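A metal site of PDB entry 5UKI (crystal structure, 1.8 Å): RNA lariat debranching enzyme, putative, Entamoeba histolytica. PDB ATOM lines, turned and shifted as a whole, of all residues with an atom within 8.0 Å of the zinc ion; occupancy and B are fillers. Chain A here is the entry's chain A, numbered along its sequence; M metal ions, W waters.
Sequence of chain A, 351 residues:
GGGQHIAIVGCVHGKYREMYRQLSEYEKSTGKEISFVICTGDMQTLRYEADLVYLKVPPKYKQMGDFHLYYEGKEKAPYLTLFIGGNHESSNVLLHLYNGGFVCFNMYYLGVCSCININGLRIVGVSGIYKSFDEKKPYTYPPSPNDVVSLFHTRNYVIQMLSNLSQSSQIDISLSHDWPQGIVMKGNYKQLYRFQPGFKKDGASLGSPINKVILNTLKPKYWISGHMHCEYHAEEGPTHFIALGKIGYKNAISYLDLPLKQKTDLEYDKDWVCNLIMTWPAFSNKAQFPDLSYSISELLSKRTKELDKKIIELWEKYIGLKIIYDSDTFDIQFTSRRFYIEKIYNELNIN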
ATOM      1  N   GLY A  10      17.907 -24.604  15.999  1.00  0.00           N
ATOM      2  CA  GLY A  10      19.174 -23.935  15.933  1.00  0.00           C
ATOM      3  C   GLY A  10      18.971 -22.410  16.170  1.00  0.00           C
ATOM      4  O   GLY A  10      18.300 -22.003  17.092  1.00  0.00           O
ATOM      5  N   CYS A  11      19.469 -21.593  15.274  1.00  0.00           N
ATOM      6  CA  CYS A  11      19.326 -20.166  15.442  1.00  0.00           C
ATOM      7  C   CYS A  11      17.956 -19.636  15.093  1.00  0.00           C
ATOM      8  O   CYS A  11      17.364 -19.980  14.058  1.00  0.00           O
ATOM      9  CB  CYS A  11      20.319 -19.459  14.535  1.00  0.00           C
ATOM     10  SG  CYS A  11      22.004 -19.859  14.750  1.00  0.00           S
ATOM     11  N   VAL A  12      17.423 -18.717  15.911  1.00  0.00           N
ATOM     12  CA  VAL A  12      16.152 -18.088  15.558  1.00  0.00           C
ATOM     13  C   VAL A  12      16.310 -16.783  14.751  1.00  0.00           C
ATOM     14  O   VAL A  12      15.573 -16.561  13.776  1.00  0.00           O
ATOM     15  CB  VAL A  12      15.263 -17.925  16.797  1.00  0.00           C
ATOM     16  CG1 VAL A  12      14.009 -17.205  16.464  1.00  0.00           C
ATOM     17  CG2 VAL A  12      14.939 -19.284  17.433  1.00  0.00           C
ATOM     18  N   HIS A  13      17.255 -15.969  15.133  1.00  0.00           N
ATOM     19  CA  HIS A  13      17.546 -14.658  14.502  1.00  0.00           C
ATOM     20  C   HIS A  13      16.258 -13.854  14.345  1.00  0.00           C
ATOM     21  O   HIS A  13      16.011 -13.288  13.321  1.00  0.00           O
ATOM     22  CB  HIS A  13      18.281 -14.864  13.167  1.00  0.00           C
ATOM     23  CG  HIS A  13      19.689 -15.293  13.334  1.00  0.00           C
ATOM     24  ND1 HIS A  13      20.677 -14.499  13.860  1.00  0.00           N
ATOM     25  CD2 HIS A  13      20.275 -16.498  13.083  1.00  0.00           C
ATOM     26  CE1 HIS A  13      21.814 -15.162  13.884  1.00  0.00           C
ATOM     27  NE2 HIS A  13      21.581 -16.365  13.407  1.00  0.00           N
ATOM     28  N   THR A  40      18.718 -23.138  20.586  1.00  0.00           N
ATOM     29  CA  THR A  40      20.122 -22.987  20.873  1.00  0.00           C
ATOM     30  C   THR A  40      20.691 -21.569  20.730  1.00  0.00           C
ATOM     31  O   THR A  40      21.879 -21.386  20.963  1.00  0.00           O
ATOM     32  CB  THR A  40      20.960 -23.966  19.969  1.00  0.00           C
ATOM     33  OG1 THR A  40      20.692 -23.691  18.610  1.00  0.00           O
ATOM     34  CG2 THR A  40      20.583 -25.352  20.220  1.00  0.00           C
ATOM     35  N   GLY A  41      19.841 -20.587  20.449  1.00  0.00           N
ATOM     36  CA  GLY A  41      20.160 -19.181  20.667  1.00  0.00           C
ATOM     37  C   GLY A  41      19.934 -18.301  19.446  1.00  0.00           C
ATOM     38  O   GLY A  41      19.182 -18.634  18.520  1.00  0.00           O
ATOM     39  N   ASP A  42      20.525 -17.116  19.512  1.00  0.00           N
ATOM     40  CA  ASP A  42      20.241 -15.966  18.625  1.00  0.00           C
ATOM     41  C   ASP A  42      18.764 -15.611  18.694  1.00  0.00           C
ATOM     42  O   ASP A  42      18.039 -15.543  17.719  1.00  0.00           O
ATOM     43  CB  ASP A  42      20.807 -16.227  17.215  1.00  0.00           C
ATOM     44  CG  ASP A  42      22.366 -16.188  17.190  1.00  0.00           C
ATOM     45  OD1 ASP A  42      22.933 -15.650  18.154  1.00  0.00           O
ATOM     46  OD2 ASP A  42      23.029 -16.751  16.249  1.00  0.00           O
ATOM     47  N   GLY A  86      22.770 -16.663  22.288  1.00  0.00           N
ATOM     48  CA  GLY A  86      23.844 -16.748  21.307  1.00  0.00           C
ATOM     49  C   GLY A  86      24.632 -15.455  21.161  1.00  0.00           C
ATOM     50  O   GLY A  86      25.007 -14.828  22.134  1.00  0.00           O
ATOM     51  N   ASN A  87      24.946 -15.108  19.927  1.00  0.00           N
ATOM     52  CA  ASN A  87      25.615 -13.846  19.628  1.00  0.00           C
ATOM     53  C   ASN A  87      24.698 -12.728  19.133  1.00  0.00           C
ATOM     54  O   ASN A  87      25.143 -11.585  19.079  1.00  0.00           O
ATOM     55  CB  ASN A  87      26.761 -14.031  18.596  1.00  0.00           C
ATOM     56  CG  ASN A  87      26.267 -14.627  17.287  1.00  0.00           C
ATOM     57  OD1 ASN A  87      25.991 -15.804  17.214  1.00  0.00           O
ATOM     58  ND2 ASN A  87      26.185 -13.816  16.241  1.00  0.00           N
ATOM     59  N   HIS A  88      23.474 -13.005  18.766  1.00  0.00           N
ATOM     60  CA  HIS A  88      22.508 -11.975  18.405  1.00  0.00           C
ATOM     61  C   HIS A  88      21.381 -11.930  19.439  1.00  0.00           C
ATOM     62  O   HIS A  88      20.381 -12.684  19.378  1.00  0.00           O
ATOM     63  CB  HIS A  88      21.876 -12.162  17.061  1.00  0.00           C
ATOM     64  CG  HIS A  88      22.793 -11.920  15.932  1.00  0.00           C
ATOM     65  ND1 HIS A  88      22.418 -12.162  14.629  1.00  0.00           N
ATOM     66  CD2 HIS A  88      24.091 -11.517  15.886  1.00  0.00           C
ATOM     67  CE1 HIS A  88      23.440 -11.873  13.818  1.00  0.00           C
ATOM     68  NE2 HIS A  88      24.461 -11.489  14.557  1.00  0.00           N
ATOM     69  N   HIS A 177      25.544 -22.702  22.094  1.00  0.00           N
ATOM     70  CA  HIS A 177      25.315 -21.986  20.885  1.00  0.00           C
ATOM     71  C   HIS A 177      26.406 -22.368  19.865  1.00  0.00           C
ATOM     72  O   HIS A 177      26.102 -22.969  18.832  1.00  0.00           O
ATOM     73  CB  HIS A 177      25.192 -20.474  21.092  1.00  0.00           C
ATOM     74  CG  HIS A 177      24.796 -19.760  19.851  1.00  0.00           C
ATOM     75  ND1 HIS A 177      23.555 -19.909  19.290  1.00  0.00           N
ATOM     76  CD2 HIS A 177      25.485 -18.944  19.023  1.00  0.00           C
ATOM     77  CE1 HIS A 177      23.485 -19.215  18.170  1.00  0.00           C
ATOM     78  NE2 HIS A 177      24.631 -18.584  18.033  1.00  0.00           N
ATOM     79  N   GLY A 226      23.949 -24.747  17.659  1.00  0.00           N
ATOM     80  CA  GLY A 226      23.521 -24.022  16.481  1.00  0.00           C
ATOM     81  C   GLY A 226      24.688 -23.194  15.929  1.00  0.00           C
ATOM     82  O   GLY A 226      25.775 -23.758  15.735  1.00  0.00           O
ATOM     83  N   HIS A 227      24.430 -21.901  15.717  1.00  0.00           N
ATOM     84  CA  HIS A 227      25.372 -20.856  15.318  1.00  0.00           C
ATOM     85  C   HIS A 227      25.946 -20.985  13.898  1.00  0.00           C
ATOM     86  O   HIS A 227      26.079 -19.996  13.224  1.00  0.00           O
ATOM     87  CB  HIS A 227      26.590 -20.776  16.287  1.00  0.00           C
ATOM     88  CG  HIS A 227      27.498 -19.621  16.060  1.00  0.00           C
ATOM     89  ND1 HIS A 227      27.071 -18.302  16.067  1.00  0.00           N
ATOM     90  CD2 HIS A 227      28.861 -19.574  15.971  1.00  0.00           C
ATOM     91  CE1 HIS A 227      28.100 -17.508  15.912  1.00  0.00           C
ATOM     92  NE2 HIS A 227      29.205 -18.255  15.878  1.00  0.00           N
ATOM     93  N   MET A 228      26.310 -22.189  13.481  1.00  0.00           N
ATOM     94  CA  MET A 228      27.082 -22.367  12.209  1.00  0.00           C
ATOM     95  C   MET A 228      26.202 -22.420  10.970  1.00  0.00           C
ATOM     96  O   MET A 228      26.723 -22.450   9.828  1.00  0.00           O
ATOM     97  CB  MET A 228      27.931 -23.625  12.335  1.00  0.00           C
ATOM     98  CG  MET A 228      28.973 -23.614  13.457  1.00  0.00           C
ATOM     99  SD  MET A 228      30.071 -22.187  13.526  1.00  0.00           S
ATOM    100  CE  MET A 228      30.878 -22.130  11.940  1.00  0.00           C
ATOM    101  N   HIS A 229      24.868 -22.470  11.137  1.00  0.00           N
ATOM    102  CA  HIS A 229      23.952 -22.475   9.981  1.00  0.00           C
ATOM    103  C   HIS A 229      24.069 -23.707   9.080  1.00  0.00           C
ATOM    104  O   HIS A 229      23.846 -23.656   7.864  1.00  0.00           O
ATOM    105  CB  HIS A 229      24.109 -21.184   9.212  1.00  0.00           C
ATOM    106  CG  HIS A 229      23.934 -19.999  10.081  1.00  0.00           C
ATOM    107  ND1 HIS A 229      24.269 -18.724   9.673  1.00  0.00           N
ATOM    108  CD2 HIS A 229      23.424 -19.875  11.329  1.00  0.00           C
ATOM    109  CE1 HIS A 229      23.949 -17.865  10.623  1.00  0.00           C
ATOM    110  NE2 HIS A 229      23.423 -18.547  11.622  1.00  0.00           N
ATOM    111  N   LEU A 244      22.344 -27.722  14.373  1.00  0.00           N
ATOM    112  CA  LEU A 244      21.139 -27.333  13.672  1.00  0.00           C
ATOM    113  C   LEU A 244      21.394 -25.976  12.996  1.00  0.00           C
ATOM    114  O   LEU A 244      22.244 -25.185  13.433  1.00  0.00           O
ATOM    115  CB  LEU A 244      19.963 -27.169  14.631  1.00  0.00           C
ATOM    116  CG  LEU A 244      19.483 -28.458  15.337  1.00  0.00           C
ATOM    117  CD1 LEU A 244      18.634 -28.143  16.544  1.00  0.00           C
ATOM    118  CD2 LEU A 244      18.788 -29.310  14.338  1.00  0.00           C
ATOM    119  N   GLY A 245      20.620 -25.761  11.932  1.00  0.00           N
ATOM    120  CA  GLY A 245      20.666 -24.582  11.093  1.00  0.00           C
ATOM    121  C   GLY A 245      19.867 -23.405  11.662  1.00  0.00           C
ATOM    122  O   GLY A 245      19.635 -23.318  12.888  1.00  0.00           O
ATOM    123  N   LYS A 246      19.476 -22.489  10.768  1.00  0.00           N
ATOM    124  CA  LYS A 246      18.769 -21.260  11.133  1.00  0.00           C
ATOM    125  C   LYS A 246      17.420 -21.179  10.495  1.00  0.00           C
ATOM    126  O   LYS A 246      17.208 -21.544   9.317  1.00  0.00           O
ATOM    127  CB  LYS A 246      19.567 -19.997  10.820  1.00  0.00           C
ATOM    128  CG  LYS A 246      19.999 -19.773   9.425  1.00  0.00           C
ATOM    129  CD  LYS A 246      20.446 -18.286   9.228  1.00  0.00           C
ATOM    130  CE  LYS A 246      21.174 -18.229   7.879  1.00  0.00           C
ATOM    131  NZ  LYS A 246      21.581 -16.876   7.298  1.00  0.00           N
ATOM    132  N   ILE A 247      16.459 -20.756  11.321  1.00  0.00           N
ATOM    133  CA  ILE A 247      15.069 -20.641  10.900  1.00  0.00           C
ATOM    134  C   ILE A 247      14.955 -19.866   9.557  1.00  0.00           C
ATOM    135  O   ILE A 247      15.537 -18.762   9.350  1.00  0.00           O
ATOM    136  CB  ILE A 247      14.178 -19.942  11.932  1.00  0.00           C
ATOM    137  CG1 ILE A 247      13.987 -20.752  13.242  1.00  0.00           C
ATOM    138  CG2 ILE A 247      12.840 -19.658  11.313  1.00  0.00           C
ATOM    139  CD1 ILE A 247      13.376 -22.110  13.063  1.00  0.00           C
HETATM  140 ZN    ZN M   1      22.889 -18.024  13.632  1.00  0.00          ZN
HETATM  141 MN    MN M   2      24.957 -17.341  16.283  1.00  0.00          MN
HETATM  142  O   HOH W   1      24.614 -17.478  14.211  1.00  0.00           O
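The zinc ion is bound by water W1 (1.9 Å), a ring nitrogen (NE2) of His 13 (2.1 Å), a ring nitrogen (NE2) of His 229 (2.1 Å) and the side-chain sulfur of Cys 11 (2.3 Å).
The backbone carbonyl oxygen of Cys 11 is in hydrogen-bond range of the backbone NH of Ile 247.
O of Asp 42 sits at hydrogen-bond distance from N of His 13, at 2.7 Å.
N of Cys 11 sits at hydrogen-bond distance from O of Gly 245 (2.9 Å).
The side-chain sulfur (SG) of Cys 11 sits close to the backbone NH (N) of His 227.
The side-chain carboxylate of Asp 42 is in hydrogen-bond range of the backbone NH of His 88 (2.8 Å).
A ring nitrogen (ND1) of His 13 lies within hydrogen-bond range of a ring nitrogen (ND1) of His 88.
A ring nitrogen (NE2) of His 229 sits close to the backbone carbonyl oxygen of His 227, at 3.4 Å.
Residues that only touch the zinc ion: Asp 42 (2.9 Å) and His 227 (3.8 Å).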
